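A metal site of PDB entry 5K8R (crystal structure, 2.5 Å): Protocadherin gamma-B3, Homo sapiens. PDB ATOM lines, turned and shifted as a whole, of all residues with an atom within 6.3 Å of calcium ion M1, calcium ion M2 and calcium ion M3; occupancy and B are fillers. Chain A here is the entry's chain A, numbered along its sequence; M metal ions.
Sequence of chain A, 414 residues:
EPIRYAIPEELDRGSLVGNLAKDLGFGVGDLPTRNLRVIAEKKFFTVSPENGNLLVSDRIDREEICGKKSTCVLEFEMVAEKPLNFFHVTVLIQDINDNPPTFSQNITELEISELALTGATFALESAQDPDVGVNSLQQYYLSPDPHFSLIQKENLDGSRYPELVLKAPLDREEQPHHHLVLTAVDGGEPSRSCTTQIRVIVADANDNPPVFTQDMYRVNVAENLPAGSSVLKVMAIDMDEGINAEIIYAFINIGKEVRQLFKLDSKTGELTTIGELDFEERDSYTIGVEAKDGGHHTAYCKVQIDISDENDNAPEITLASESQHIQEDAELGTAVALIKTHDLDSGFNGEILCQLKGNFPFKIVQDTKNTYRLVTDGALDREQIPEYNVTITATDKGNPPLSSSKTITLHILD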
ATOM      1  N   GLU A   9     -15.838  29.421  22.647  1.00  0.00           N
ATOM      2  CA  GLU A   9     -16.226  30.657  21.998  1.00  0.00           C
ATOM      3  C   GLU A   9     -16.087  31.837  22.951  1.00  0.00           C
ATOM      4  O   GLU A   9     -15.872  31.683  24.164  1.00  0.00           O
ATOM      5  CB  GLU A   9     -17.669  30.566  21.486  1.00  0.00           C
ATOM      6  CG  GLU A   9     -18.665  30.179  22.573  1.00  0.00           C
ATOM      7  CD  GLU A   9     -20.111  30.389  22.146  1.00  0.00           C
ATOM      8  OE1 GLU A   9     -20.371  31.281  21.312  1.00  0.00           O
ATOM      9  OE2 GLU A   9     -20.986  29.656  22.644  1.00  0.00           O
ATOM     10  N   GLU A  10     -16.194  33.041  22.393  1.00  0.00           N
ATOM     11  CA  GLU A  10     -16.226  34.290  23.154  1.00  0.00           C
ATOM     12  C   GLU A  10     -14.956  34.526  23.961  1.00  0.00           C
ATOM     13  O   GLU A  10     -14.986  35.129  25.036  1.00  0.00           O
ATOM     14  CB  GLU A  10     -17.457  34.339  24.082  1.00  0.00           C
ATOM     15  CG  GLU A  10     -18.780  34.089  23.380  1.00  0.00           C
ATOM     16  CD  GLU A  10     -19.238  35.266  22.538  1.00  0.00           C
ATOM     17  OE1 GLU A  10     -18.593  36.336  22.600  1.00  0.00           O
ATOM     18  OE2 GLU A  10     -20.248  35.122  21.818  1.00  0.00           O
ATOM     19  N   ARG A  59     -14.055  38.749  17.874  1.00  0.00           N
ATOM     20  CA  ARG A  59     -15.032  37.995  18.631  1.00  0.00           C
ATOM     21  C   ARG A  59     -15.506  36.785  17.844  1.00  0.00           C
ATOM     22  O   ARG A  59     -15.912  36.902  16.676  1.00  0.00           O
ATOM     23  CB  ARG A  59     -16.229  38.886  18.996  1.00  0.00           C
ATOM     24  CG  ARG A  59     -17.348  38.146  19.695  1.00  0.00           C
ATOM     25  CD  ARG A  59     -18.386  39.105  20.245  1.00  0.00           C
ATOM     26  NE  ARG A  59     -19.463  38.406  20.944  1.00  0.00           N
ATOM     27  CZ  ARG A  59     -20.651  38.123  20.406  1.00  0.00           C
ATOM     28  NH1 ARG A  59     -20.920  38.488  19.164  1.00  0.00           N
ATOM     29  NH2 ARG A  59     -21.562  37.479  21.114  1.00  0.00           N
ATOM     30  N   ILE A  60     -15.455  35.614  18.468  1.00  0.00           N
ATOM     31  CA  ILE A  60     -15.912  34.383  17.852  1.00  0.00           C
ATOM     32  C   ILE A  60     -17.195  33.929  18.535  1.00  0.00           C
ATOM     33  O   ILE A  60     -17.148  33.234  19.564  1.00  0.00           O
ATOM     34  CB  ILE A  60     -14.827  33.283  17.905  1.00  0.00           C
ATOM     35  CG1 ILE A  60     -13.548  33.774  17.225  1.00  0.00           C
ATOM     36  CG2 ILE A  60     -15.318  31.999  17.250  1.00  0.00           C
ATOM     37  CD1 ILE A  60     -12.430  32.763  17.222  1.00  0.00           C
ATOM     38  N   ASP A  61     -18.338  34.331  18.002  1.00  0.00           N
ATOM     39  CA  ASP A  61     -19.636  33.965  18.542  1.00  0.00           C
ATOM     40  C   ASP A  61     -20.143  32.728  17.815  1.00  0.00           C
ATOM     41  O   ASP A  61     -20.466  32.793  16.618  1.00  0.00           O
ATOM     42  CB  ASP A  61     -20.617  35.126  18.410  1.00  0.00           C
ATOM     43  CG  ASP A  61     -22.024  34.759  18.843  1.00  0.00           C
ATOM     44  OD1 ASP A  61     -22.173  33.880  19.717  1.00  0.00           O
ATOM     45  OD2 ASP A  61     -22.992  35.354  18.310  1.00  0.00           O
ATOM     46  N   ARG A  62     -20.215  31.604  18.523  1.00  0.00           N
ATOM     47  CA  ARG A  62     -20.641  30.357  17.895  1.00  0.00           C
ATOM     48  C   ARG A  62     -22.085  30.421  17.423  1.00  0.00           C
ATOM     49  O   ARG A  62     -22.446  29.775  16.428  1.00  0.00           O
ATOM     50  CB  ARG A  62     -20.448  29.190  18.855  1.00  0.00           C
ATOM     51  CG  ARG A  62     -20.602  27.820  18.211  1.00  0.00           C
ATOM     52  CD  ARG A  62     -21.228  26.828  19.169  1.00  0.00           C
ATOM     53  NE  ARG A  62     -22.551  27.258  19.604  1.00  0.00           N
ATOM     54  CZ  ARG A  62     -23.659  27.069  18.894  1.00  0.00           C
ATOM     55  NH1 ARG A  62     -23.614  26.456  17.720  1.00  0.00           N
ATOM     56  NH2 ARG A  62     -24.827  27.504  19.358  1.00  0.00           N
ATOM     57  N   GLU A  63     -22.938  31.182  18.127  1.00  0.00           N
ATOM     58  CA  GLU A  63     -24.332  31.292  17.719  1.00  0.00           C
ATOM     59  C   GLU A  63     -24.470  31.988  16.366  1.00  0.00           C
ATOM     60  O   GLU A  63     -25.298  31.591  15.541  1.00  0.00           O
ATOM     61  CB  GLU A  63     -25.134  32.037  18.786  1.00  0.00           C
ATOM     62  CG  GLU A  63     -25.592  31.168  19.942  1.00  0.00           C
ATOM     63  CD  GLU A  63     -24.444  30.709  20.822  1.00  0.00           C
ATOM     64  OE1 GLU A  63     -23.594  31.544  21.184  1.00  0.00           O
ATOM     65  OE2 GLU A  63     -24.390  29.503  21.140  1.00  0.00           O
ATOM     66  N   GLU A  64     -23.662  33.012  16.126  1.00  0.00           N
ATOM     67  CA  GLU A  64     -23.737  33.733  14.856  1.00  0.00           C
ATOM     68  C   GLU A  64     -23.026  32.986  13.730  1.00  0.00           C
ATOM     69  O   GLU A  64     -23.389  33.136  12.566  1.00  0.00           O
ATOM     70  CB  GLU A  64     -23.155  35.139  15.017  1.00  0.00           C
ATOM     71  CG  GLU A  64     -23.372  36.043  13.810  1.00  0.00           C
ATOM     72  CD  GLU A  64     -22.805  37.429  14.037  1.00  0.00           C
ATOM     73  OE1 GLU A  64     -22.158  37.652  15.086  1.00  0.00           O
ATOM     74  OE2 GLU A  64     -22.995  38.299  13.152  1.00  0.00           O
ATOM     75  N   ASP A  95     -19.111  25.286  22.453  1.00  0.00           N
ATOM     76  CA  ASP A  95     -20.255  26.101  22.874  1.00  0.00           C
ATOM     77  C   ASP A  95     -20.218  26.326  24.377  1.00  0.00           C
ATOM     78  O   ASP A  95     -19.951  25.402  25.157  1.00  0.00           O
ATOM     79  CB  ASP A  95     -21.569  25.412  22.477  1.00  0.00           C
ATOM     80  CG  ASP A  95     -22.787  26.231  22.882  1.00  0.00           C
ATOM     81  OD1 ASP A  95     -22.797  27.463  22.636  1.00  0.00           O
ATOM     82  OD2 ASP A  95     -23.734  25.642  23.440  1.00  0.00           O
ATOM     83  N   ILE A  96     -20.505  27.566  24.783  1.00  0.00           N
ATOM     84  CA  ILE A  96     -20.677  27.912  26.185  1.00  0.00           C
ATOM     85  C   ILE A  96     -22.117  28.358  26.387  1.00  0.00           C
ATOM     86  O   ILE A  96     -22.798  28.799  25.462  1.00  0.00           O
ATOM     87  CB  ILE A  96     -19.683  28.998  26.650  1.00  0.00           C
ATOM     88  CG1 ILE A  96     -19.965  30.320  25.923  1.00  0.00           C
ATOM     89  CG2 ILE A  96     -18.254  28.546  26.421  1.00  0.00           C
ATOM     90  CD1 ILE A  96     -19.020  31.445  26.327  1.00  0.00           C
ATOM     91  N   ASN A  97     -22.583  28.243  27.632  1.00  0.00           N
ATOM     92  CA  ASN A  97     -23.962  28.598  27.978  1.00  0.00           C
ATOM     93  C   ASN A  97     -24.013  30.088  28.310  1.00  0.00           C
ATOM     94  O   ASN A  97     -24.117  30.498  29.475  1.00  0.00           O
ATOM     95  CB  ASN A  97     -24.471  27.746  29.135  1.00  0.00           C
ATOM     96  CG  ASN A  97     -25.954  27.928  29.381  1.00  0.00           C
ATOM     97  OD1 ASN A  97     -26.724  28.152  28.451  1.00  0.00           O
ATOM     98  ND2 ASN A  97     -26.361  27.852  30.637  1.00  0.00           N
ATOM     99  N   ASP A  98     -23.937  30.916  27.274  1.00  0.00           N
ATOM    100  CA  ASP A  98     -23.988  32.361  27.418  1.00  0.00           C
ATOM    101  C   ASP A  98     -25.293  32.958  26.894  1.00  0.00           C
ATOM    102  O   ASP A  98     -25.373  34.171  26.709  1.00  0.00           O
ATOM    103  CB  ASP A  98     -22.788  33.003  26.714  1.00  0.00           C
ATOM    104  CG  ASP A  98     -22.716  32.651  25.250  1.00  0.00           C
ATOM    105  OD1 ASP A  98     -23.295  31.619  24.850  1.00  0.00           O
ATOM    106  OD2 ASP A  98     -22.074  33.412  24.488  1.00  0.00           O
ATOM    107  N   ASN A  99     -26.300  32.130  26.659  1.00  0.00           N
ATOM    108  CA  ASN A  99     -27.593  32.590  26.178  1.00  0.00           C
ATOM    109  C   ASN A  99     -28.691  31.960  27.029  1.00  0.00           C
ATOM    110  O   ASN A  99     -28.705  30.731  27.211  1.00  0.00           O
ATOM    111  CB  ASN A  99     -27.806  32.237  24.701  1.00  0.00           C
ATOM    112  CG  ASN A  99     -26.976  33.099  23.770  1.00  0.00           C
ATOM    113  OD1 ASN A  99     -26.088  32.600  23.080  1.00  0.00           O
ATOM    114  ND2 ASN A  99     -27.266  34.397  23.754  1.00  0.00           N
ATOM    115  N   PRO A 100     -29.620  32.749  27.566  1.00  0.00           N
ATOM    116  CA  PRO A 100     -30.713  32.186  28.334  1.00  0.00           C
ATOM    117  C   PRO A 100     -31.825  31.703  27.417  1.00  0.00           C
ATOM    118  O   PRO A 100     -31.912  32.135  26.260  1.00  0.00           O
ATOM    119  CB  PRO A 100     -31.177  33.371  29.190  1.00  0.00           C
ATOM    120  CG  PRO A 100     -30.917  34.555  28.322  1.00  0.00           C
ATOM    121  CD  PRO A 100     -29.660  34.225  27.548  1.00  0.00           C
ATOM    122  N   PRO A 101     -32.691  30.805  27.897  1.00  0.00           N
ATOM    123  CA  PRO A 101     -33.876  30.458  27.120  1.00  0.00           C
ATOM    124  C   PRO A 101     -34.824  31.639  27.033  1.00  0.00           C
ATOM    125  O   PRO A 101     -34.709  32.629  27.761  1.00  0.00           O
ATOM    126  CB  PRO A 101     -34.506  29.309  27.923  1.00  0.00           C
ATOM    127  CG  PRO A 101     -33.982  29.492  29.318  1.00  0.00           C
ATOM    128  CD  PRO A 101     -32.601  30.047  29.158  1.00  0.00           C
ATOM    129  N   ASP A 129     -33.681  28.427  22.629  1.00  0.00           N
ATOM    130  CA  ASP A 129     -32.344  28.684  23.147  1.00  0.00           C
ATOM    131  C   ASP A 129     -31.334  28.587  22.002  1.00  0.00           C
ATOM    132  O   ASP A 129     -31.174  27.515  21.401  1.00  0.00           O
ATOM    133  CB  ASP A 129     -31.997  27.692  24.256  1.00  0.00           C
ATOM    134  CG  ASP A 129     -30.855  28.165  25.131  1.00  0.00           C
ATOM    135  OD1 ASP A 129     -29.828  28.614  24.578  1.00  0.00           O
ATOM    136  OD2 ASP A 129     -30.982  28.071  26.368  1.00  0.00           O
ATOM    137  N   PRO A 130     -30.632  29.681  21.669  1.00  0.00           N
ATOM    138  CA  PRO A 130     -29.693  29.635  20.547  1.00  0.00           C
ATOM    139  C   PRO A 130     -28.456  28.800  20.800  1.00  0.00           C
ATOM    140  O   PRO A 130     -27.666  28.587  19.867  1.00  0.00           O
ATOM    141  CB  PRO A 130     -29.332  31.115  20.325  1.00  0.00           C
ATOM    142  CG  PRO A 130     -29.558  31.742  21.660  1.00  0.00           C
ATOM    143  CD  PRO A 130     -30.712  31.020  22.280  1.00  0.00           C
ATOM    144  N   ASP A 131     -28.246  28.326  22.034  1.00  0.00           N
ATOM    145  CA  ASP A 131     -27.125  27.444  22.314  1.00  0.00           C
ATOM    146  C   ASP A 131     -27.405  26.052  21.741  1.00  0.00           C
ATOM    147  O   ASP A 131     -28.444  25.793  21.131  1.00  0.00           O
ATOM    148  CB  ASP A 131     -26.870  27.370  23.818  1.00  0.00           C
ATOM    149  CG  ASP A 131     -26.453  28.717  24.400  1.00  0.00           C
ATOM    150  OD1 ASP A 131     -25.810  29.502  23.676  1.00  0.00           O
ATOM    151  OD2 ASP A 131     -26.776  28.975  25.583  1.00  0.00           O
ATOM    152  N   VAL A 132     -26.456  25.139  21.935  1.00  0.00           N
ATOM    153  CA  VAL A 132     -26.566  23.765  21.466  1.00  0.00           C
ATOM    154  C   VAL A 132     -26.156  22.816  22.574  1.00  0.00           C
ATOM    155  O   VAL A 132     -25.604  23.229  23.607  1.00  0.00           O
ATOM    156  CB  VAL A 132     -25.716  23.517  20.194  1.00  0.00           C
ATOM    157  CG1 VAL A 132     -26.313  24.255  19.002  1.00  0.00           C
ATOM    158  CG2 VAL A 132     -24.283  23.931  20.426  1.00  0.00           C
ATOM    159  N   VAL A 134     -26.258  20.462  25.764  1.00  0.00           N
ATOM    160  CA  VAL A 134     -26.954  20.617  27.042  1.00  0.00           C
ATOM    161  C   VAL A 134     -27.224  22.071  27.366  1.00  0.00           C
ATOM    162  O   VAL A 134     -28.098  22.364  28.200  1.00  0.00           O
ATOM    163  CB  VAL A 134     -26.140  19.954  28.170  1.00  0.00           C
ATOM    164  CG1 VAL A 134     -26.004  18.458  27.923  1.00  0.00           C
ATOM    165  CG2 VAL A 134     -24.778  20.604  28.300  1.00  0.00           C
ATOM    166  N   ASN A 135     -26.505  23.002  26.728  1.00  0.00           N
ATOM    167  CA  ASN A 135     -26.722  24.419  26.999  1.00  0.00           C
ATOM    168  C   ASN A 135     -28.071  24.909  26.485  1.00  0.00           C
ATOM    169  O   ASN A 135     -28.534  25.969  26.908  1.00  0.00           O
ATOM    170  CB  ASN A 135     -25.596  25.246  26.382  1.00  0.00           C
ATOM    171  CG  ASN A 135     -24.239  24.874  26.913  1.00  0.00           C
ATOM    172  OD1 ASN A 135     -24.111  24.365  28.033  1.00  0.00           O
ATOM    173  ND2 ASN A 135     -23.199  25.114  26.116  1.00  0.00           N
ATOM    174  N   SER A 136     -28.714  24.153  25.589  1.00  0.00           N
ATOM    175  CA  SER A 136     -30.053  24.481  25.117  1.00  0.00           C
ATOM    176  C   SER A 136     -31.101  23.454  25.545  1.00  0.00           C
ATOM    177  O   SER A 136     -32.289  23.681  25.296  1.00  0.00           O
ATOM    178  CB  SER A 136     -30.076  24.611  23.592  1.00  0.00           C
ATOM    179  OG  SER A 136     -29.683  23.399  22.976  1.00  0.00           O
ATOM    180  N   GLN A 138     -33.733  22.090  27.664  1.00  0.00           N
ATOM    181  CA  GLN A 138     -34.562  22.819  28.598  1.00  0.00           C
ATOM    182  C   GLN A 138     -35.240  21.897  29.605  1.00  0.00           C
ATOM    183  O   GLN A 138     -35.444  20.703  29.353  1.00  0.00           O
ATOM    184  CB  GLN A 138     -35.628  23.637  27.856  1.00  0.00           C
ATOM    185  CG  GLN A 138     -35.058  24.647  26.882  1.00  0.00           C
ATOM    186  CD  GLN A 138     -34.086  25.612  27.539  1.00  0.00           C
ATOM    187  OE1 GLN A 138     -34.287  26.032  28.685  1.00  0.00           O
ATOM    188  NE2 GLN A 138     -33.020  25.946  26.830  1.00  0.00           N
ATOM    189  N   ASP A 186     -32.224  25.941  31.455  1.00  0.00           N
ATOM    190  CA  ASP A 186     -31.380  25.131  30.597  1.00  0.00           C
ATOM    191  C   ASP A 186     -30.429  24.269  31.429  1.00  0.00           C
ATOM    192  O   ASP A 186     -30.385  24.361  32.657  1.00  0.00           O
ATOM    193  CB  ASP A 186     -30.607  26.020  29.609  1.00  0.00           C
ATOM    194  CG  ASP A 186     -29.812  27.116  30.289  1.00  0.00           C
ATOM    195  OD1 ASP A 186     -29.387  26.944  31.460  1.00  0.00           O
ATOM    196  OD2 ASP A 186     -29.591  28.164  29.650  1.00  0.00           O
ATOM    197  N   GLY A 187     -29.665  23.417  30.752  1.00  0.00           N
ATOM    198  CA  GLY A 187     -28.764  22.518  31.439  1.00  0.00           C
ATOM    199  C   GLY A 187     -27.301  22.893  31.295  1.00  0.00           C
ATOM    200  O   GLY A 187     -26.428  22.038  31.392  1.00  0.00           O
ATOM    201  N   GLY A 188     -27.028  24.177  31.045  1.00  0.00           N
ATOM    202  CA  GLY A 188     -25.680  24.650  30.875  1.00  0.00           C
ATOM    203  C   GLY A 188     -25.067  25.142  32.174  1.00  0.00           C
ATOM    204  O   GLY A 188     -25.647  25.061  33.253  1.00  0.00           O
ATOM    205  N   ARG A 192     -29.235  29.002  33.235  1.00  0.00           N
ATOM    206  CA  ARG A 192     -29.993  30.189  32.843  1.00  0.00           C
ATOM    207  C   ARG A 192     -31.453  29.809  32.653  1.00  0.00           C
ATOM    208  O   ARG A 192     -31.760  28.704  32.186  1.00  0.00           O
ATOM    209  CB  ARG A 192     -29.433  30.801  31.554  1.00  0.00           C
ATOM    210  CG  ARG A 192     -28.077  31.474  31.744  1.00  0.00           C
ATOM    211  CD  ARG A 192     -27.534  32.006  30.426  1.00  0.00           C
ATOM    212  NE  ARG A 192     -26.791  33.249  30.610  1.00  0.00           N
ATOM    213  CZ  ARG A 192     -25.511  33.310  30.978  1.00  0.00           C
ATOM    214  NH1 ARG A 192     -24.833  32.196  31.200  1.00  0.00           N
ATOM    215  NH2 ARG A 192     -24.919  34.490  31.115  1.00  0.00           N
HETATM  216 CA    CA M   1     -28.713  28.361  27.061  1.00  0.00          CA
HETATM  217 CA    CA M   2     -23.375  29.696  23.316  1.00  0.00          CA
HETATM  218 CA    CA M   3     -22.077  33.253  22.051  1.00  0.00          CA
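The side-chain carboxylate (OD2) of Asp 129 lies close to the side-chain amide nitrogen (NE2) of Gln 138 (3.0 Å). ND2 of Asn 135 lies within hydrogen-bond range of OD2 of Asp 95 (2.8 Å). The side-chain carboxylate (OD1) of Asp 95 lies close to the guanidinium group (NE) of Arg 62, 3.0 Å away. The side-chain carboxylate (OE2) of Glu 63 lies close to the guanidinium group (NH2) of Arg 62, at 2.7 Å. N of Glu 64 lies within hydrogen-bond range of OD2 of Asp 61, at 3.3 Å. The backbone carbonyl oxygen of Asp 131 lies close to the side-chain hydroxyl of Ser 136 (3.3 Å). OE1 of Glu 9 sits close to N of Arg 62. The backbone NH (N) of Asp 186 sits at hydrogen-bond distance from the side-chain amide oxygen (OE1) of Gln 138, 3.5 Å away.
Within 4 Å of calcium ion M1: Asn 97, Asn 99, Asp 129, Asp 131, Asn 135 and Asp 186. The nearest printed residue that does not touch calcium ion M1 is Ser 136 (4.5 Å).
Within 4 Å of calcium ion M2: Glu 9, Glu 63, Asp 95, Ile 96, Asp 98, Asn 99 and Asp 131. The nearest printed residue that does not touch calcium ion M2 is Arg 62 (4.5 Å).
The nearest printed residue that does not touch calcium ion M3 is Asn 99 (4.2 Å).
Calcium ion M1 is bound by the backbone carbonyl oxygen (O) of Asn 99, 2.4 Å away. OD2 of Asp 129 is bound to calcium ion M1. Calcium ion M1 is bound by O of Asn 135 (2.4 Å). OD1 of Asn 97 is bound to calcium ion M1. OD2 of Asp 131 binds calcium ion M1. OD1 of Asp 129 binds calcium ion M1, at 2.7 Å. OD2 of Asp 186 is bound to calcium ion M1.
Calcium ion M2 is bound by the backbone carbonyl oxygen (O) of Ile 96 (2.4 Å), the side-chain carboxylate (OD1) of Asp 95 (2.4 Å), the side-chain carboxylate (OE2) of Glu 63 (2.4 Å), the side-chain carboxylate (OD1) of Asp 98 (2.5 Å), the side-chain carboxylate (OD1) of Asp 131 (2.5 Å), the side-chain carboxylate (OE2) of Glu 9 (2.5 Å) and the side-chain carboxylate (OE1) of Glu 63 (2.8 Å).
OD1 of Asp 61 binds calcium ion M3. OD2 of Asp 98 is bound to calcium ion M3 (2.4 Å). The side-chain carboxylate (OE1) of Glu 63 is bound to calcium ion M3. The side-chain carboxylate (OE2) of Glu 10 is bound to calcium ion M3 (2.6 Å). The side-chain carboxylate (OE1) of Glu 9 is bound to calcium ion M3 (2.7 Å).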
